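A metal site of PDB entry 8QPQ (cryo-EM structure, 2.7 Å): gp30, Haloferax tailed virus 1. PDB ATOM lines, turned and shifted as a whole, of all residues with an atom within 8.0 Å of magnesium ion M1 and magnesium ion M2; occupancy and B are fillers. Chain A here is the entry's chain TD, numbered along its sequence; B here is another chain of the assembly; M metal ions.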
ATOM      1  N   ASP A  29      -4.076  10.253  22.220  1.00  0.00           N
ATOM      2  CA  ASP A  29      -4.783  10.468  20.976  1.00  0.00           C
ATOM      3  C   ASP A  29      -5.976  11.378  21.239  1.00  0.00           C
ATOM      4  O   ASP A  29      -6.875  11.035  21.998  1.00  0.00           O
ATOM      5  CB  ASP A  29      -5.200   9.102  20.442  1.00  0.00           C
ATOM      6  CG  ASP A  29      -5.803   9.154  19.055  1.00  0.00           C
ATOM      7  OD1 ASP A  29      -6.092  10.263  18.557  1.00  0.00           O
ATOM      8  OD2 ASP A  29      -6.001   8.058  18.479  1.00  0.00           O
ATOM      9  N   PRO A  30      -6.051  12.585  20.625  1.00  0.00           N
ATOM     10  CA  PRO A  30      -7.209  13.451  20.801  1.00  0.00           C
ATOM     11  C   PRO A  30      -8.496  12.913  20.170  1.00  0.00           C
ATOM     12  O   PRO A  30      -9.541  13.453  20.427  1.00  0.00           O
ATOM     13  CB  PRO A  30      -6.791  14.787  20.182  1.00  0.00           C
ATOM     14  CG  PRO A  30      -5.800  14.358  19.126  1.00  0.00           C
ATOM     15  CD  PRO A  30      -5.049  13.194  19.757  1.00  0.00           C
ATOM     16  N   GLN A  31      -8.432  11.790  19.423  1.00  0.00           N
ATOM     17  CA  GLN A  31      -9.628  11.083  18.980  1.00  0.00           C
ATOM     18  C   GLN A  31     -10.426  10.492  20.136  1.00  0.00           C
ATOM     19  O   GLN A  31     -11.627  10.230  19.976  1.00  0.00           O
ATOM     20  CB  GLN A  31      -9.246   9.972  18.003  1.00  0.00           C
ATOM     21  CG  GLN A  31      -8.688  10.498  16.705  1.00  0.00           C
ATOM     22  CD  GLN A  31      -8.267   9.389  15.776  1.00  0.00           C
ATOM     23  OE1 GLN A  31      -8.961   9.066  14.825  1.00  0.00           O
ATOM     24  NE2 GLN A  31      -7.114   8.799  16.024  1.00  0.00           N
ATOM     25  N   GLY A  36     -12.682  16.221  20.442  1.00  0.00           N
ATOM     26  CA  GLY A  36     -11.661  15.897  19.456  1.00  0.00           C
ATOM     27  C   GLY A  36     -10.399  16.757  19.548  1.00  0.00           C
ATOM     28  O   GLY A  36      -9.550  16.664  18.676  1.00  0.00           O
ATOM     29  N   SER A  56       0.311  13.197  12.053  1.00  0.00           N
ATOM     30  CA  SER A  56       0.101  12.061  11.169  1.00  0.00           C
ATOM     31  C   SER A  56      -0.242  12.496   9.731  1.00  0.00           C
ATOM     32  O   SER A  56      -0.955  13.476   9.529  1.00  0.00           O
ATOM     33  CB  SER A  56      -0.970  11.164  11.699  1.00  0.00           C
ATOM     34  OG  SER A  56      -1.058  10.021  10.864  1.00  0.00           O
ATOM     35  N   ASP A  58      -2.200  10.404   8.168  1.00  0.00           N
ATOM     36  CA  ASP A  58      -3.510   9.774   8.119  1.00  0.00           C
ATOM     37  C   ASP A  58      -4.489  10.427   9.101  1.00  0.00           C
ATOM     38  O   ASP A  58      -4.115  10.829  10.197  1.00  0.00           O
ATOM     39  CB  ASP A  58      -3.345   8.274   8.379  1.00  0.00           C
ATOM     40  CG  ASP A  58      -4.643   7.496   8.301  1.00  0.00           C
ATOM     41  OD1 ASP A  58      -5.451   7.566   9.254  1.00  0.00           O
ATOM     42  OD2 ASP A  58      -4.878   6.884   7.249  1.00  0.00           O
ATOM     43  N   ASP A  59      -5.770  10.523   8.729  1.00  0.00           N
ATOM     44  CA  ASP A  59      -6.765  11.209   9.530  1.00  0.00           C
ATOM     45  C   ASP A  59      -7.080  10.536  10.866  1.00  0.00           C
ATOM     46  O   ASP A  59      -7.598  11.192  11.784  1.00  0.00           O
ATOM     47  CB  ASP A  59      -8.059  11.442   8.752  1.00  0.00           C
ATOM     48  CG  ASP A  59      -7.932  12.560   7.731  1.00  0.00           C
ATOM     49  OD1 ASP A  59      -7.037  13.428   7.917  1.00  0.00           O
ATOM     50  OD2 ASP A  59      -8.727  12.568   6.769  1.00  0.00           O
ATOM     51  N   THR A  60      -6.777   9.229  10.973  1.00  0.00           N
ATOM     52  CA  THR A  60      -7.326   8.347  12.002  1.00  0.00           C
ATOM     53  C   THR A  60      -6.262   7.508  12.702  1.00  0.00           C
ATOM     54  O   THR A  60      -6.461   7.092  13.838  1.00  0.00           O
ATOM     55  CB  THR A  60      -8.377   7.421  11.385  1.00  0.00           C
ATOM     56  OG1 THR A  60      -7.771   6.675  10.335  1.00  0.00           O
ATOM     57  CG2 THR A  60      -9.585   8.155  10.851  1.00  0.00           C
ATOM     58  N   GLU A  61      -5.135   7.250  12.016  1.00  0.00           N
ATOM     59  CA  GLU A  61      -4.036   6.436  12.542  1.00  0.00           C
ATOM     60  C   GLU A  61      -2.755   7.262  12.563  1.00  0.00           C
ATOM     61  O   GLU A  61      -2.618   8.224  11.796  1.00  0.00           O
ATOM     62  CB  GLU A  61      -3.840   5.201  11.657  1.00  0.00           C
ATOM     63  CG  GLU A  61      -5.063   4.300  11.620  1.00  0.00           C
ATOM     64  CD  GLU A  61      -4.871   2.962  10.923  1.00  0.00           C
ATOM     65  OE1 GLU A  61      -3.930   2.855  10.101  1.00  0.00           O
ATOM     66  OE2 GLU A  61      -5.665   2.029  11.191  1.00  0.00           O
ATOM     67  N   SER A  87      -5.167  17.878  18.329  1.00  0.00           N
ATOM     68  CA  SER A  87      -6.516  17.649  17.820  1.00  0.00           C
ATOM     69  C   SER A  87      -6.542  16.505  16.822  1.00  0.00           C
ATOM     70  O   SER A  87      -5.546  16.198  16.169  1.00  0.00           O
ATOM     71  CB  SER A  87      -7.147  18.883  17.231  1.00  0.00           C
ATOM     72  OG  SER A  87      -6.759  19.071  15.875  1.00  0.00           O
ATOM     73  N   ASP A  88      -7.728  15.910  16.688  1.00  0.00           N
ATOM     74  CA  ASP A  88      -7.982  14.910  15.679  1.00  0.00           C
ATOM     75  C   ASP A  88      -7.887  15.518  14.281  1.00  0.00           C
ATOM     76  O   ASP A  88      -7.203  14.964  13.426  1.00  0.00           O
ATOM     77  CB  ASP A  88      -9.326  14.239  15.881  1.00  0.00           C
ATOM     78  CG  ASP A  88      -9.594  13.180  14.812  1.00  0.00           C
ATOM     79  OD1 ASP A  88      -8.674  12.841  14.017  1.00  0.00           O
ATOM     80  OD2 ASP A  88     -10.746  12.714  14.767  1.00  0.00           O
ATOM     81  N   ASN A  89      -8.566  16.637  14.012  1.00  0.00           N
ATOM     82  CA  ASN A  89      -8.623  17.146  12.658  1.00  0.00           C
ATOM     83  C   ASN A  89      -7.265  17.626  12.146  1.00  0.00           C
ATOM     84  O   ASN A  89      -6.964  17.480  10.967  1.00  0.00           O
ATOM     85  CB  ASN A  89      -9.721  18.189  12.500  1.00  0.00           C
ATOM     86  CG  ASN A  89      -9.892  18.638  11.074  1.00  0.00           C
ATOM     87  OD1 ASN A  89     -10.200  17.823  10.211  1.00  0.00           O
ATOM     88  ND2 ASN A  89      -9.658  19.903  10.814  1.00  0.00           N
ATOM     89  N   THR A  90      -6.416  18.158  13.033  1.00  0.00           N
ATOM     90  CA  THR A  90      -5.039  18.483  12.664  1.00  0.00           C
ATOM     91  C   THR A  90      -4.083  17.307  12.869  1.00  0.00           C
ATOM     92  O   THR A  90      -2.861  17.472  12.800  1.00  0.00           O
ATOM     93  CB  THR A  90      -4.532  19.759  13.343  1.00  0.00           C
ATOM     94  OG1 THR A  90      -4.318  19.548  14.736  1.00  0.00           O
ATOM     95  CG2 THR A  90      -5.492  20.917  13.200  1.00  0.00           C
ATOM     96  N   ASN A  91      -4.634  16.114  13.144  1.00  0.00           N
ATOM     97  CA  ASN A  91      -3.908  14.838  13.172  1.00  0.00           C
ATOM     98  C   ASN A  91      -2.685  14.850  14.074  1.00  0.00           C
ATOM     99  O   ASN A  91      -1.629  14.344  13.731  1.00  0.00           O
ATOM    100  CB  ASN A  91      -3.667  14.369  11.746  1.00  0.00           C
ATOM    101  CG  ASN A  91      -4.973  14.005  11.086  1.00  0.00           C
ATOM    102  OD1 ASN A  91      -5.831  13.389  11.719  1.00  0.00           O
ATOM    103  ND2 ASN A  91      -5.161  14.395   9.853  1.00  0.00           N
ATOM    104  N   THR A  92      -2.832  15.501  15.239  1.00  0.00           N
ATOM    105  CA  THR A  92      -1.723  15.711  16.157  1.00  0.00           C
ATOM    106  C   THR A  92      -1.822  14.700  17.299  1.00  0.00           C
ATOM    107  O   THR A  92      -2.874  14.527  17.868  1.00  0.00           O
ATOM    108  CB  THR A  92      -1.730  17.168  16.644  1.00  0.00           C
ATOM    109  OG1 THR A  92      -1.526  18.009  15.515  1.00  0.00           O
ATOM    110  CG2 THR A  92      -0.586  17.488  17.573  1.00  0.00           C
ATOM    111  N   TYR A  93      -0.695  14.085  17.649  1.00  0.00           N
ATOM    112  CA  TYR A  93      -0.611  13.060  18.686  1.00  0.00           C
ATOM    113  C   TYR A  93       0.502  13.436  19.649  1.00  0.00           C
ATOM    114  O   TYR A  93       1.485  14.056  19.250  1.00  0.00           O
ATOM    115  CB  TYR A  93      -0.295  11.691  18.072  1.00  0.00           C
ATOM    116  CG  TYR A  93      -1.362  11.079  17.201  1.00  0.00           C
ATOM    117  CD1 TYR A  93      -1.562  11.519  15.889  1.00  0.00           C
ATOM    118  CD2 TYR A  93      -2.190  10.078  17.688  1.00  0.00           C
ATOM    119  CE1 TYR A  93      -2.557  10.998  15.087  1.00  0.00           C
ATOM    120  CE2 TYR A  93      -3.182   9.526  16.878  1.00  0.00           C
ATOM    121  CZ  TYR A  93      -3.365   9.975  15.576  1.00  0.00           C
ATOM    122  OH  TYR A  93      -4.380   9.474  14.809  1.00  0.00           O
ATOM    123  N   GLN A 115     -12.611  21.827  18.847  1.00  0.00           N
ATOM    124  CA  GLN A 115     -12.002  22.086  17.545  1.00  0.00           C
ATOM    125  C   GLN A 115     -12.650  23.339  16.903  1.00  0.00           C
ATOM    126  O   GLN A 115     -12.203  23.702  15.776  1.00  0.00           O
ATOM    127  CB  GLN A 115     -12.047  20.836  16.680  1.00  0.00           C
ATOM    128  CG  GLN A 115     -11.115  19.759  17.202  1.00  0.00           C
ATOM    129  CD  GLN A 115     -11.239  18.457  16.444  1.00  0.00           C
ATOM    130  OE1 GLN A 115     -10.354  18.044  15.713  1.00  0.00           O
ATOM    131  NE2 GLN A 115     -12.362  17.781  16.631  1.00  0.00           N
ATOM    132  OXT GLN A 115     -13.543  23.934  17.562  1.00  0.00           O
ATOM    133  N   ASN B 231     -17.780  19.589  -0.462  1.00  0.00           N
ATOM    134  CA  ASN B 231     -17.588  19.006   0.859  1.00  0.00           C
ATOM    135  C   ASN B 231     -17.591  20.135   1.889  1.00  0.00           C
ATOM    136  O   ASN B 231     -16.856  21.094   1.726  1.00  0.00           O
ATOM    137  CB  ASN B 231     -16.271  18.199   0.863  1.00  0.00           C
ATOM    138  CG  ASN B 231     -15.865  17.735   2.220  1.00  0.00           C
ATOM    139  OD1 ASN B 231     -16.395  16.793   2.745  1.00  0.00           O
ATOM    140  ND2 ASN B 231     -14.910  18.476   2.793  1.00  0.00           N
ATOM    141  N   ASP B 233     -16.232  20.495   5.526  1.00  0.00           N
ATOM    142  CA  ASP B 233     -15.439  19.948   6.599  1.00  0.00           C
ATOM    143  C   ASP B 233     -15.843  20.643   7.912  1.00  0.00           C
ATOM    144  O   ASP B 233     -15.530  21.816   8.118  1.00  0.00           O
ATOM    145  CB  ASP B 233     -13.956  20.073   6.287  1.00  0.00           C
ATOM    146  CG  ASP B 233     -13.046  19.340   7.253  1.00  0.00           C
ATOM    147  OD1 ASP B 233     -13.560  18.834   8.299  1.00  0.00           O
ATOM    148  OD2 ASP B 233     -11.850  19.299   6.992  1.00  0.00           O
ATOM    149  N   THR B 234     -16.514  19.895   8.795  1.00  0.00           N
ATOM    150  CA  THR B 234     -16.954  20.440  10.066  1.00  0.00           C
ATOM    151  C   THR B 234     -15.800  20.598  11.057  1.00  0.00           C
ATOM    152  O   THR B 234     -15.948  21.328  12.015  1.00  0.00           O
ATOM    153  CB  THR B 234     -18.097  19.614  10.668  1.00  0.00           C
ATOM    154  OG1 THR B 234     -17.660  18.319  11.053  1.00  0.00           O
ATOM    155  CG2 THR B 234     -19.284  19.465   9.764  1.00  0.00           C
ATOM    156  N   ALA B 235     -14.703  19.839  10.867  1.00  0.00           N
ATOM    157  CA  ALA B 235     -13.537  19.855  11.746  1.00  0.00           C
ATOM    158  C   ALA B 235     -13.931  19.601  13.216  1.00  0.00           C
ATOM    159  O   ALA B 235     -13.533  20.333  14.104  1.00  0.00           O
ATOM    160  CB  ALA B 235     -12.794  21.167  11.552  1.00  0.00           C
ATOM    161  N   GLY B 236     -14.819  18.635  13.450  1.00  0.00           N
ATOM    162  CA  GLY B 236     -15.333  18.297  14.755  1.00  0.00           C
ATOM    163  C   GLY B 236     -16.119  19.400  15.456  1.00  0.00           C
ATOM    164  O   GLY B 236     -16.221  19.353  16.692  1.00  0.00           O
ATOM    165  N   SER B 334     -15.316   9.952  13.597  1.00  0.00           N
ATOM    166  CA  SER B 334     -13.878  10.164  13.487  1.00  0.00           C
ATOM    167  C   SER B 334     -13.542  11.032  12.285  1.00  0.00           C
ATOM    168  O   SER B 334     -14.284  11.094  11.313  1.00  0.00           O
ATOM    169  CB  SER B 334     -13.209   8.829  13.422  1.00  0.00           C
ATOM    170  OG  SER B 334     -13.711   8.058  12.343  1.00  0.00           O
ATOM    171  N   ASP B 335     -12.414  11.746  12.353  1.00  0.00           N
ATOM    172  CA  ASP B 335     -11.975  12.704  11.340  1.00  0.00           C
ATOM    173  C   ASP B 335     -11.992  12.098   9.929  1.00  0.00           C
ATOM    174  O   ASP B 335     -11.398  11.055   9.680  1.00  0.00           O
ATOM    175  CB  ASP B 335     -10.574  13.150  11.743  1.00  0.00           C
ATOM    176  CG  ASP B 335      -9.792  14.102  10.844  1.00  0.00           C
ATOM    177  OD1 ASP B 335     -10.406  14.826  10.054  1.00  0.00           O
ATOM    178  OD2 ASP B 335      -8.563  14.078  10.930  1.00  0.00           O
ATOM    179  N   GLY B 336     -12.694  12.771   9.006  1.00  0.00           N
ATOM    180  CA  GLY B 336     -12.753  12.355   7.610  1.00  0.00           C
ATOM    181  C   GLY B 336     -13.944  11.468   7.289  1.00  0.00           C
ATOM    182  O   GLY B 336     -14.198  11.207   6.111  1.00  0.00           O
ATOM    183  N   ASP B 337     -14.711  11.012   8.311  1.00  0.00           N
ATOM    184  CA  ASP B 337     -15.972  10.335   8.075  1.00  0.00           C
ATOM    185  C   ASP B 337     -16.963  11.263   7.357  1.00  0.00           C
ATOM    186  O   ASP B 337     -17.074  12.442   7.680  1.00  0.00           O
ATOM    187  CB  ASP B 337     -16.629   9.905   9.381  1.00  0.00           C
ATOM    188  CG  ASP B 337     -15.938   8.825  10.196  1.00  0.00           C
ATOM    189  OD1 ASP B 337     -15.039   8.162   9.640  1.00  0.00           O
ATOM    190  OD2 ASP B 337     -16.340   8.635  11.371  1.00  0.00           O
ATOM    191  N   GLN B 395     -18.528  16.358   6.437  1.00  0.00           N
ATOM    192  CA  GLN B 395     -17.372  15.603   6.894  1.00  0.00           C
ATOM    193  C   GLN B 395     -17.079  15.941   8.351  1.00  0.00           C
ATOM    194  O   GLN B 395     -17.090  17.106   8.727  1.00  0.00           O
ATOM    195  CB  GLN B 395     -16.190  15.898   5.967  1.00  0.00           C
ATOM    196  CG  GLN B 395     -14.906  15.210   6.401  1.00  0.00           C
ATOM    197  CD  GLN B 395     -13.730  15.565   5.528  1.00  0.00           C
ATOM    198  OE1 GLN B 395     -12.578  15.516   5.954  1.00  0.00           O
ATOM    199  NE2 GLN B 395     -13.978  15.932   4.290  1.00  0.00           N
ATOM    200  N   TYR B 396     -16.821  14.915   9.153  1.00  0.00           N
ATOM    201  CA  TYR B 396     -16.423  15.047  10.549  1.00  0.00           C
ATOM    202  C   TYR B 396     -14.998  15.618  10.684  1.00  0.00           C
ATOM    203  O   TYR B 396     -14.084  15.079  10.058  1.00  0.00           O
ATOM    204  CB  TYR B 396     -16.547  13.668  11.194  1.00  0.00           C
ATOM    205  CG  TYR B 396     -16.522  13.665  12.693  1.00  0.00           C
ATOM    206  CD1 TYR B 396     -15.324  13.780  13.399  1.00  0.00           C
ATOM    207  CD2 TYR B 396     -17.700  13.530  13.423  1.00  0.00           C
ATOM    208  CE1 TYR B 396     -15.302  13.765  14.789  1.00  0.00           C
ATOM    209  CE2 TYR B 396     -17.685  13.506  14.804  1.00  0.00           C
ATOM    210  CZ  TYR B 396     -16.495  13.640  15.497  1.00  0.00           C
ATOM    211  OH  TYR B 396     -16.477  13.628  16.862  1.00  0.00           O
ATOM    212  OXT TYR B 396     -14.833  16.610  11.441  1.00  0.00           O
HETATM  213 MG    MG M   1      -7.632  13.159  12.433  1.00  0.00          MG
HETATM  214 MG    MG M   2     -10.377  16.554   8.735  1.00  0.00          MG
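N of Asp 88 is in hydrogen-bond range of O of Gly 36 (2.8 Å).
OD1 of Asn 91 lies close to O of Asp 58, at 3.4 Å.
The backbone carbonyl oxygen (O) of Asn 91 sits at hydrogen-bond distance from the backbone NH (N) of Ser 56 (2.8 Å).
N of Asn 89 is in hydrogen-bond range of OE1 of Gln 115.
The side-chain carboxylate of Asp 233 of chain B lies within hydrogen-bond range of the backbone NH of Ala 235 of chain B (3.0 Å).
The backbone carbonyl oxygen (O) of Gln 395 of chain B is in hydrogen-bond range of the side-chain hydroxyl (OG1) of Thr 234 of chain B, 2.7 Å away.
Of the 28 residues printed, 5 come within 4 Å of magnesium ion M1.
The nearest printed residue that does not touch magnesium ion M1 is Thr 60 (4.3 Å).
OD2 of Asp 233 of chain B touches magnesium ion M2, 3.6 Å away.
Gln 395 of chain B touches magnesium ion M2.
Of the 28 residues printed, 4 come within 4 Å of magnesium ion M2.
The nearest printed residue that does not touch magnesium ion M2 is Tyr 396 of chain B (4.2 Å).
Magnesium ion M1 is bound by OD1 of Asp 88, OD1 of Asn 91, OD2 of Asp 335 of chain B, O of Asp 59 and O of Asp 88.
Magnesium ion M1 has five donor atoms within binding distance.
Magnesium ion M2 is bound by the side-chain amide oxygen (OD1) of Asn 89 and the side-chain carboxylate (OD1) of Asp 335 of chain B.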
